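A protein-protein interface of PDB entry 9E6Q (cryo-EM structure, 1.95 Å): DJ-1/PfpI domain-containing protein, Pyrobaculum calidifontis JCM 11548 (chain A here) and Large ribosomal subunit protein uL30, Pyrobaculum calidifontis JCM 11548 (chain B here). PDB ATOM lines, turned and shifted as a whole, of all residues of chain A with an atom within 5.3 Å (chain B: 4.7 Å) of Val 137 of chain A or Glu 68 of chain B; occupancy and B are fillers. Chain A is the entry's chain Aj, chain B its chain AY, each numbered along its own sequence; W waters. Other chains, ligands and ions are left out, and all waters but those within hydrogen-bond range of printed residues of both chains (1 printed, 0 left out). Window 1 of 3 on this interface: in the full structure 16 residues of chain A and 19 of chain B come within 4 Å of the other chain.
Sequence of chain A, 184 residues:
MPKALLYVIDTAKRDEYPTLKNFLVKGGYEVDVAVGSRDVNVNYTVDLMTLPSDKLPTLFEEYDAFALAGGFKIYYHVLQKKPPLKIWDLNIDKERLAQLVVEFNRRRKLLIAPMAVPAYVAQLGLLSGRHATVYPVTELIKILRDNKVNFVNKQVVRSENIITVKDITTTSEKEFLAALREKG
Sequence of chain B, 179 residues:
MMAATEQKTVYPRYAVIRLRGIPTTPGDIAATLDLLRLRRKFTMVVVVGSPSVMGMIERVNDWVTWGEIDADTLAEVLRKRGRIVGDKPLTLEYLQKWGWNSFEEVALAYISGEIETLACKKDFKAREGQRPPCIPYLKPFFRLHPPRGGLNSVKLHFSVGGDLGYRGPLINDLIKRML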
ATOM      1  N   TYR A  75     -19.165 -12.146 -11.837  1.00  0.00           N
ATOM      2  CA  TYR A  75     -17.982 -11.535 -12.429  1.00  0.00           C
ATOM      3  C   TYR A  75     -17.944 -10.036 -12.174  1.00  0.00           C
ATOM      4  O   TYR A  75     -16.898  -9.484 -11.825  1.00  0.00           O
ATOM      5  CB  TYR A  75     -17.938 -11.865 -13.927  1.00  0.00           C
ATOM      6  CG  TYR A  75     -16.915 -11.119 -14.757  1.00  0.00           C
ATOM      7  CD1 TYR A  75     -17.057  -9.770 -15.049  1.00  0.00           C
ATOM      8  CD2 TYR A  75     -15.778 -11.763 -15.213  1.00  0.00           C
ATOM      9  CE1 TYR A  75     -16.119  -9.103 -15.792  1.00  0.00           C
ATOM     10  CE2 TYR A  75     -14.836 -11.101 -15.946  1.00  0.00           C
ATOM     11  CZ  TYR A  75     -15.011  -9.769 -16.232  1.00  0.00           C
ATOM     12  OH  TYR A  75     -14.065  -9.106 -16.973  1.00  0.00           O
ATOM     13  N   TYR A  76     -19.078  -9.358 -12.333  1.00  0.00           N
ATOM     14  CA  TYR A  76     -19.084  -7.913 -12.157  1.00  0.00           C
ATOM     15  C   TYR A  76     -19.262  -7.496 -10.709  1.00  0.00           C
ATOM     16  O   TYR A  76     -18.969  -6.347 -10.373  1.00  0.00           O
ATOM     17  CB  TYR A  76     -20.159  -7.282 -13.040  1.00  0.00           C
ATOM     18  CG  TYR A  76     -19.696  -7.169 -14.469  1.00  0.00           C
ATOM     19  CD1 TYR A  76     -18.819  -6.169 -14.850  1.00  0.00           C
ATOM     20  CD2 TYR A  76     -20.102  -8.082 -15.423  1.00  0.00           C
ATOM     21  CE1 TYR A  76     -18.376  -6.070 -16.141  1.00  0.00           C
ATOM     22  CE2 TYR A  76     -19.664  -7.991 -16.720  1.00  0.00           C
ATOM     23  CZ  TYR A  76     -18.799  -6.982 -17.074  1.00  0.00           C
ATOM     24  OH  TYR A  76     -18.362  -6.885 -18.364  1.00  0.00           O
ATOM     25  N   LYS A  81     -17.656  -3.471 -10.752  1.00  0.00           N
ATOM     26  CA  LYS A  81     -17.728  -2.754 -12.012  1.00  0.00           C
ATOM     27  C   LYS A  81     -19.159  -2.789 -12.530  1.00  0.00           C
ATOM     28  O   LYS A  81     -19.926  -3.699 -12.212  1.00  0.00           O
ATOM     29  CB  LYS A  81     -16.776  -3.374 -13.035  1.00  0.00           C
ATOM     30  CG  LYS A  81     -16.397  -2.477 -14.188  1.00  0.00           C
ATOM     31  CD  LYS A  81     -15.628  -3.257 -15.246  1.00  0.00           C
ATOM     32  CE  LYS A  81     -15.727  -2.600 -16.615  1.00  0.00           C
ATOM     33  NZ  LYS A  81     -17.062  -1.997 -16.869  1.00  0.00           N
ATOM     34  N   TYR A 135     -11.074 -17.867 -14.114  1.00  0.00           N
ATOM     35  CA  TYR A 135     -11.205 -17.384 -15.480  1.00  0.00           C
ATOM     36  C   TYR A 135     -10.060 -16.422 -15.758  1.00  0.00           C
ATOM     37  O   TYR A 135     -10.018 -15.329 -15.186  1.00  0.00           O
ATOM     38  CB  TYR A 135     -12.547 -16.698 -15.692  1.00  0.00           C
ATOM     39  CG  TYR A 135     -12.921 -16.544 -17.137  1.00  0.00           C
ATOM     40  CD1 TYR A 135     -13.070 -17.649 -17.952  1.00  0.00           C
ATOM     41  CD2 TYR A 135     -13.122 -15.293 -17.687  1.00  0.00           C
ATOM     42  CE1 TYR A 135     -13.412 -17.516 -19.271  1.00  0.00           C
ATOM     43  CE2 TYR A 135     -13.465 -15.146 -19.006  1.00  0.00           C
ATOM     44  CZ  TYR A 135     -13.609 -16.264 -19.795  1.00  0.00           C
ATOM     45  OH  TYR A 135     -13.953 -16.135 -21.114  1.00  0.00           O
ATOM     46  N   PRO A 136      -9.125 -16.785 -16.622  1.00  0.00           N
ATOM     47  CA  PRO A 136      -7.827 -16.097 -16.660  1.00  0.00           C
ATOM     48  C   PRO A 136      -7.878 -14.761 -17.390  1.00  0.00           C
ATOM     49  O   PRO A 136      -7.252 -14.565 -18.428  1.00  0.00           O
ATOM     50  CB  PRO A 136      -6.934 -17.120 -17.374  1.00  0.00           C
ATOM     51  CG  PRO A 136      -7.847 -18.052 -18.081  1.00  0.00           C
ATOM     52  CD  PRO A 136      -9.264 -17.758 -17.711  1.00  0.00           C
ATOM     53  N   VAL A 137      -8.621 -13.818 -16.836  1.00  0.00           N
ATOM     54  CA  VAL A 137      -8.552 -12.447 -17.291  1.00  0.00           C
ATOM     55  C   VAL A 137      -7.704 -11.669 -16.299  1.00  0.00           C
ATOM     56  O   VAL A 137      -7.509 -12.078 -15.156  1.00  0.00           O
ATOM     57  CB  VAL A 137      -9.942 -11.801 -17.476  1.00  0.00           C
ATOM     58  CG1 VAL A 137     -10.677 -12.463 -18.628  1.00  0.00           C
ATOM     59  CG2 VAL A 137     -10.748 -11.879 -16.204  1.00  0.00           C
ATOM     60  N   THR A 138      -7.185 -10.530 -16.755  1.00  0.00           N
ATOM     61  CA  THR A 138      -6.192  -9.784 -15.991  1.00  0.00           C
ATOM     62  C   THR A 138      -6.692  -9.438 -14.598  1.00  0.00           C
ATOM     63  O   THR A 138      -5.994  -9.651 -13.603  1.00  0.00           O
ATOM     64  CB  THR A 138      -5.818  -8.506 -16.736  1.00  0.00           C
ATOM     65  OG1 THR A 138      -5.161  -8.839 -17.962  1.00  0.00           O
ATOM     66  CG2 THR A 138      -4.902  -7.652 -15.887  1.00  0.00           C
ATOM     67  N   GLU A 139      -7.906  -8.901 -14.510  1.00  0.00           N
ATOM     68  CA  GLU A 139      -8.407  -8.414 -13.234  1.00  0.00           C
ATOM     69  C   GLU A 139      -8.714  -9.548 -12.269  1.00  0.00           C
ATOM     70  O   GLU A 139      -8.533  -9.390 -11.060  1.00  0.00           O
ATOM     71  CB  GLU A 139      -9.644  -7.555 -13.462  1.00  0.00           C
ATOM     72  CG  GLU A 139      -9.340  -6.198 -14.052  1.00  0.00           C
ATOM     73  CD  GLU A 139     -10.504  -5.621 -14.827  1.00  0.00           C
ATOM     74  OE1 GLU A 139     -11.101  -4.634 -14.356  1.00  0.00           O
ATOM     75  OE2 GLU A 139     -10.821  -6.147 -15.914  1.00  0.00           O
ATOM     76  N   LEU A 140      -9.196 -10.684 -12.770  1.00  0.00           N
ATOM     77  CA  LEU A 140      -9.538 -11.788 -11.879  1.00  0.00           C
ATOM     78  C   LEU A 140      -8.290 -12.474 -11.346  1.00  0.00           C
ATOM     79  O   LEU A 140      -8.264 -12.915 -10.194  1.00  0.00           O
ATOM     80  CB  LEU A 140     -10.433 -12.790 -12.599  1.00  0.00           C
ATOM     81  CG  LEU A 140     -11.880 -12.365 -12.843  1.00  0.00           C
ATOM     82  CD1 LEU A 140     -12.649 -13.493 -13.497  1.00  0.00           C
ATOM     83  CD2 LEU A 140     -12.555 -11.926 -11.560  1.00  0.00           C
ATOM     84  N   ILE A 141      -7.251 -12.585 -12.173  1.00  0.00           N
ATOM     85  CA  ILE A 141      -5.982 -13.130 -11.705  1.00  0.00           C
ATOM     86  C   ILE A 141      -5.405 -12.247 -10.612  1.00  0.00           C
ATOM     87  O   ILE A 141      -4.848 -12.737  -9.625  1.00  0.00           O
ATOM     88  CB  ILE A 141      -5.001 -13.287 -12.881  1.00  0.00           C
ATOM     89  CG1 ILE A 141      -5.494 -14.353 -13.855  1.00  0.00           C
ATOM     90  CG2 ILE A 141      -3.624 -13.649 -12.381  1.00  0.00           C
ATOM     91  CD1 ILE A 141      -4.793 -14.325 -15.177  1.00  0.00           C
ATOM     92  N   LYS A 142      -5.533 -10.932 -10.768  1.00  0.00           N
ATOM     93  CA  LYS A 142      -5.016 -10.007  -9.768  1.00  0.00           C
ATOM     94  C   LYS A 142      -5.749 -10.145  -8.441  1.00  0.00           C
ATOM     95  O   LYS A 142      -5.133 -10.049  -7.376  1.00  0.00           O
ATOM     96  CB  LYS A 142      -5.120  -8.578 -10.286  1.00  0.00           C
ATOM     97  CG  LYS A 142      -4.112  -7.634  -9.690  1.00  0.00           C
ATOM     98  CD  LYS A 142      -4.691  -6.247  -9.537  1.00  0.00           C
ATOM     99  CE  LYS A 142      -3.748  -5.347  -8.762  1.00  0.00           C
ATOM    100  NZ  LYS A 142      -3.914  -5.515  -7.299  1.00  0.00           N
ATOM    101  N   ARG B  13      -6.197  -6.196 -20.006  1.00  0.00           N
ATOM    102  CA  ARG B  13      -5.926  -6.436 -21.417  1.00  0.00           C
ATOM    103  C   ARG B  13      -7.236  -6.689 -22.147  1.00  0.00           C
ATOM    104  O   ARG B  13      -8.014  -7.556 -21.748  1.00  0.00           O
ATOM    105  CB  ARG B  13      -4.982  -7.622 -21.600  1.00  0.00           C
ATOM    106  CG  ARG B  13      -3.516  -7.265 -21.545  1.00  0.00           C
ATOM    107  CD  ARG B  13      -3.065  -6.976 -20.132  1.00  0.00           C
ATOM    108  NE  ARG B  13      -1.613  -6.980 -20.028  1.00  0.00           N
ATOM    109  CZ  ARG B  13      -0.894  -5.989 -19.527  1.00  0.00           C
ATOM    110  NH1 ARG B  13      -1.462  -4.900 -19.043  1.00  0.00           N
ATOM    111  NH2 ARG B  13       0.428  -6.094 -19.509  1.00  0.00           N
ATOM    112  N   TYR B  14      -7.469  -5.941 -23.217  1.00  0.00           N
ATOM    113  CA  TYR B  14      -8.720  -5.987 -23.951  1.00  0.00           C
ATOM    114  C   TYR B  14      -8.489  -6.476 -25.370  1.00  0.00           C
ATOM    115  O   TYR B  14      -7.456  -6.201 -25.975  1.00  0.00           O
ATOM    116  CB  TYR B  14      -9.378  -4.612 -24.005  1.00  0.00           C
ATOM    117  CG  TYR B  14      -9.809  -4.080 -22.671  1.00  0.00           C
ATOM    118  CD1 TYR B  14     -10.847  -4.666 -21.977  1.00  0.00           C
ATOM    119  CD2 TYR B  14      -9.187  -2.983 -22.112  1.00  0.00           C
ATOM    120  CE1 TYR B  14     -11.249  -4.181 -20.768  1.00  0.00           C
ATOM    121  CE2 TYR B  14      -9.582  -2.491 -20.901  1.00  0.00           C
ATOM    122  CZ  TYR B  14     -10.615  -3.095 -20.232  1.00  0.00           C
ATOM    123  OH  TYR B  14     -11.018  -2.609 -19.016  1.00  0.00           O
ATOM    124  N   GLY B  67     -13.810  -6.365 -25.163  1.00  0.00           N
ATOM    125  CA  GLY B  67     -14.001  -6.896 -23.828  1.00  0.00           C
ATOM    126  C   GLY B  67     -12.705  -7.465 -23.302  1.00  0.00           C
ATOM    127  O   GLY B  67     -11.676  -7.464 -23.982  1.00  0.00           O
ATOM    128  N   GLU B  68     -12.771  -7.965 -22.073  1.00  0.00           N
ATOM    129  CA  GLU B  68     -11.605  -8.543 -21.417  1.00  0.00           C
ATOM    130  C   GLU B  68     -11.305  -9.912 -22.007  1.00  0.00           C
ATOM    131  O   GLU B  68     -12.139 -10.815 -21.941  1.00  0.00           O
ATOM    132  CB  GLU B  68     -11.849  -8.663 -19.917  1.00  0.00           C
ATOM    133  CG  GLU B  68     -12.077  -7.347 -19.216  1.00  0.00           C
ATOM    134  CD  GLU B  68     -13.542  -6.971 -19.149  1.00  0.00           C
ATOM    135  OE1 GLU B  68     -14.390  -7.821 -19.465  1.00  0.00           O
ATOM    136  OE2 GLU B  68     -13.848  -5.820 -18.786  1.00  0.00           O
ATOM    137  N   ILE B  69     -10.122 -10.071 -22.566  1.00  0.00           N
ATOM    138  CA  ILE B  69      -9.725 -11.326 -23.193  1.00  0.00           C
ATOM    139  C   ILE B  69      -9.063 -12.213 -22.150  1.00  0.00           C
ATOM    140  O   ILE B  69      -8.309 -11.736 -21.299  1.00  0.00           O
ATOM    141  CB  ILE B  69      -8.796 -11.068 -24.396  1.00  0.00           C
ATOM    142  CG1 ILE B  69      -8.293 -12.385 -24.982  1.00  0.00           C
ATOM    143  CG2 ILE B  69      -7.640 -10.177 -24.005  1.00  0.00           C
ATOM    144  CD1 ILE B  69      -7.941 -12.319 -26.432  1.00  0.00           C
ATOM    145  N   ASP B  70      -9.367 -13.506 -22.192  1.00  0.00           N
ATOM    146  CA  ASP B  70      -8.791 -14.455 -21.253  1.00  0.00           C
ATOM    147  C   ASP B  70      -7.592 -15.152 -21.879  1.00  0.00           C
ATOM    148  O   ASP B  70      -7.468 -15.240 -23.100  1.00  0.00           O
ATOM    149  CB  ASP B  70      -9.826 -15.480 -20.788  1.00  0.00           C
ATOM    150  CG  ASP B  70     -10.140 -16.527 -21.831  1.00  0.00           C
ATOM    151  OD1 ASP B  70      -9.321 -17.442 -22.035  1.00  0.00           O
ATOM    152  OD2 ASP B  70     -11.218 -16.451 -22.446  1.00  0.00           O
ATOM    153  N   ILE B 111      -1.438 -11.577 -20.480  1.00  0.00           N
ATOM    154  CA  ILE B 111      -2.685 -11.269 -19.794  1.00  0.00           C
ATOM    155  C   ILE B 111      -2.413 -10.891 -18.347  1.00  0.00           C
ATOM    156  O   ILE B 111      -2.993  -9.934 -17.823  1.00  0.00           O
ATOM    157  CB  ILE B 111      -3.662 -12.452 -19.901  1.00  0.00           C
ATOM    158  CG1 ILE B 111      -4.015 -12.711 -21.365  1.00  0.00           C
ATOM    159  CG2 ILE B 111      -4.913 -12.186 -19.108  1.00  0.00           C
ATOM    160  CD1 ILE B 111      -4.623 -11.534 -22.065  1.00  0.00           C
ATOM    161  N   TYR B 166     -18.964  -2.286 -25.812  1.00  0.00           N
ATOM    162  CA  TYR B 166     -18.386  -3.107 -24.761  1.00  0.00           C
ATOM    163  C   TYR B 166     -19.198  -4.379 -24.562  1.00  0.00           C
ATOM    164  O   TYR B 166     -20.416  -4.332 -24.396  1.00  0.00           O
ATOM    165  CB  TYR B 166     -18.322  -2.308 -23.463  1.00  0.00           C
ATOM    166  CG  TYR B 166     -17.805  -3.073 -22.280  1.00  0.00           C
ATOM    167  CD1 TYR B 166     -16.526  -3.588 -22.273  1.00  0.00           C
ATOM    168  CD2 TYR B 166     -18.597  -3.275 -21.163  1.00  0.00           C
ATOM    169  CE1 TYR B 166     -16.046  -4.278 -21.196  1.00  0.00           C
ATOM    170  CE2 TYR B 166     -18.126  -3.970 -20.077  1.00  0.00           C
ATOM    171  CZ  TYR B 166     -16.848  -4.471 -20.102  1.00  0.00           C
ATOM    172  OH  TYR B 166     -16.368  -5.165 -19.025  1.00  0.00           O
ATOM    173  N   GLY B 168     -17.748  -7.114 -22.480  1.00  0.00           N
ATOM    174  CA  GLY B 168     -17.290  -7.802 -21.302  1.00  0.00           C
ATOM    175  C   GLY B 168     -16.593  -9.094 -21.649  1.00  0.00           C
ATOM    176  O   GLY B 168     -15.983  -9.226 -22.710  1.00  0.00           O
ATOM    177  N   PRO B 169     -16.677 -10.083 -20.759  1.00  0.00           N
ATOM    178  CA  PRO B 169     -16.024 -11.372 -21.028  1.00  0.00           C
ATOM    179  C   PRO B 169     -16.628 -12.130 -22.190  1.00  0.00           C
ATOM    180  O   PRO B 169     -16.026 -13.107 -22.639  1.00  0.00           O
ATOM    181  CB  PRO B 169     -16.201 -12.146 -19.719  1.00  0.00           C
ATOM    182  CG  PRO B 169     -16.836 -11.228 -18.771  1.00  0.00           C
ATOM    183  CD  PRO B 169     -17.433 -10.094 -19.504  1.00  0.00           C
ATOM    184  N   ILE B 171     -16.609 -11.305 -25.117  1.00  0.00           N
ATOM    185  CA  ILE B 171     -15.735 -11.183 -26.276  1.00  0.00           C
ATOM    186  C   ILE B 171     -15.009 -12.495 -26.536  1.00  0.00           C
ATOM    187  O   ILE B 171     -14.636 -12.791 -27.674  1.00  0.00           O
ATOM    188  CB  ILE B 171     -14.752 -10.011 -26.092  1.00  0.00           C
ATOM    189  CG1 ILE B 171     -14.118  -9.625 -27.426  1.00  0.00           C
ATOM    190  CG2 ILE B 171     -13.675 -10.354 -25.095  1.00  0.00           C
ATOM    191  CD1 ILE B 171     -14.996  -8.784 -28.297  1.00  0.00           C
ATOM    192  N   ASN B 172     -14.806 -13.306 -25.498  1.00  0.00           N
ATOM    193  CA  ASN B 172     -14.130 -14.583 -25.684  1.00  0.00           C
ATOM    194  C   ASN B 172     -15.033 -15.591 -26.375  1.00  0.00           C
ATOM    195  O   ASN B 172     -14.567 -16.390 -27.191  1.00  0.00           O
ATOM    196  CB  ASN B 172     -13.647 -15.110 -24.340  1.00  0.00           C
ATOM    197  CG  ASN B 172     -12.694 -14.165 -23.671  1.00  0.00           C
ATOM    198  OD1 ASN B 172     -11.621 -13.885 -24.190  1.00  0.00           O
ATOM    199  ND2 ASN B 172     -13.091 -13.636 -22.533  1.00  0.00           N
HETATM  200  O   HOH W   1      -8.022  -9.570 -19.755  1.00  0.00           O
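Among the printed residues, merely in contact across the chains: Pro 136 of chain A with Asp 70 of chain B, Tyr 76 of chain A with Gly 168 of chain B, Pro 136 of chain A with Ile 111 of chain B, Tyr 75 of chain A with Pro 169 of chain B, Tyr 76 of chain A with Pro 169 of chain B, Lys 81 of chain A with Tyr 166 of chain B, Val 137 of chain A with Ile 69 of chain B, Glu 139 of chain A with Glu 68 of chain B, Val 137 of chain A with Asp 70 of chain B, Tyr 135 of chain A with Pro 169 of chain B, Val 137 of chain A with Glu 68 of chain B and Val 137 of chain A with Ile 111 of chain B.
The backbone NH of Arg 13 of chain B is in hydrogen-bond range of the side-chain hydroxyl of Thr 138 of chain A (3.5 Å).
OE1 of Glu 68 of chain B sits at hydrogen-bond distance from OH of Tyr 75 of chain A, at 2.8 Å.
The side-chain hydroxyl of Tyr 135 of chain A sits at hydrogen-bond distance from the side-chain carboxylate of Asp 70 of chain B, at 3.1 Å.
The backbone carbonyl oxygen (O) of Ile 111 of chain B is in hydrogen-bond range of the side-chain hydroxyl (OG1) of Thr 138 of chain A, 2.4 Å away.
OH of Tyr 166 of chain B lies within hydrogen-bond range of OH of Tyr 76 of chain A (2.7 Å).
The side-chain amide nitrogen of Asn 172 of chain B lies within hydrogen-bond range of the side-chain hydroxyl of Tyr 135 of chain A.
Of the 11 printed residues of chain A, 8 touch a printed residue of chain B.
Among the printed residues, no Asp or Glu carboxylate lies within 4 Å of a Lys or Arg side-chain nitrogen of the other chain.
The backbone carbonyl oxygen (O) of Arg 13 of chain B is in hydrogen-bond range of the backbone NH (N) of Ile 69 of chain B.
The side-chain carboxylate (OE2) of Glu 68 of chain B is in hydrogen-bond range of the side-chain hydroxyl (OH) of Tyr 166 of chain B, 2.6 Å away.
The backbone carbonyl oxygen (O) of Glu 68 of chain B lies within hydrogen-bond range of the side-chain amide nitrogen (ND2) of Asn 172 of chain B (3.0 Å).
OD1 of Asn 172 of chain B lies within hydrogen-bond range of N of Asp 70 of chain B (3.0 Å).
The backbone carbonyl oxygen (O) of Pro 169 of chain B lies within hydrogen-bond range of the side-chain amide nitrogen (ND2) of Asn 172 of chain B (3.0 Å).
N of Lys 81 of chain A sits at hydrogen-bond distance from O of Tyr 76 of chain A, at 3.2 Å.
Water W1 lies within hydrogen-bond range of O of Ile 69 of chain B (2.7 Å), O of Arg 13 of chain B (2.8 Å) and N of Thr 138 of chain A (3.3 Å).
Printed residues of chain B within 4 Å of Val 137 of chain A: Glu 68, Ile 69, Asp 70 and Ile 111.
Glu 68 of chain B touches three residues of chain A.
Of the printed residues of chain B, Lys 81 of chain A touches Tyr 166.
Printed residues of chain B within 4 Å of Glu 139 of chain A: Glu 68 (3.7 Å).
Printed residues of chain B within 4 Å of Pro 136 of chain A: Asp 70 (3.2 Å) and Ile 111 (3.4 Å).
Of the printed residues of chain B, Tyr 135 of chain A touches Asp 70 (3.1 Å), Pro 169 (3.97 Å) and Asn 172 (3.0 Å).
Ile 141 of chain A touches none of the printed residues of chain B.
The nearest printed residue of chain B that does not touch Val 137 of chain A is Asn 172 of chain B (4.7 Å).
The nearest residue of chain A that does not touch Glu 68 of chain B is Tyr 76 of chain A (4.2 Å).
The nearest printed residue of chain B that does not touch Tyr 76 of chain A is Glu 68 of chain B (4.2 Å).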
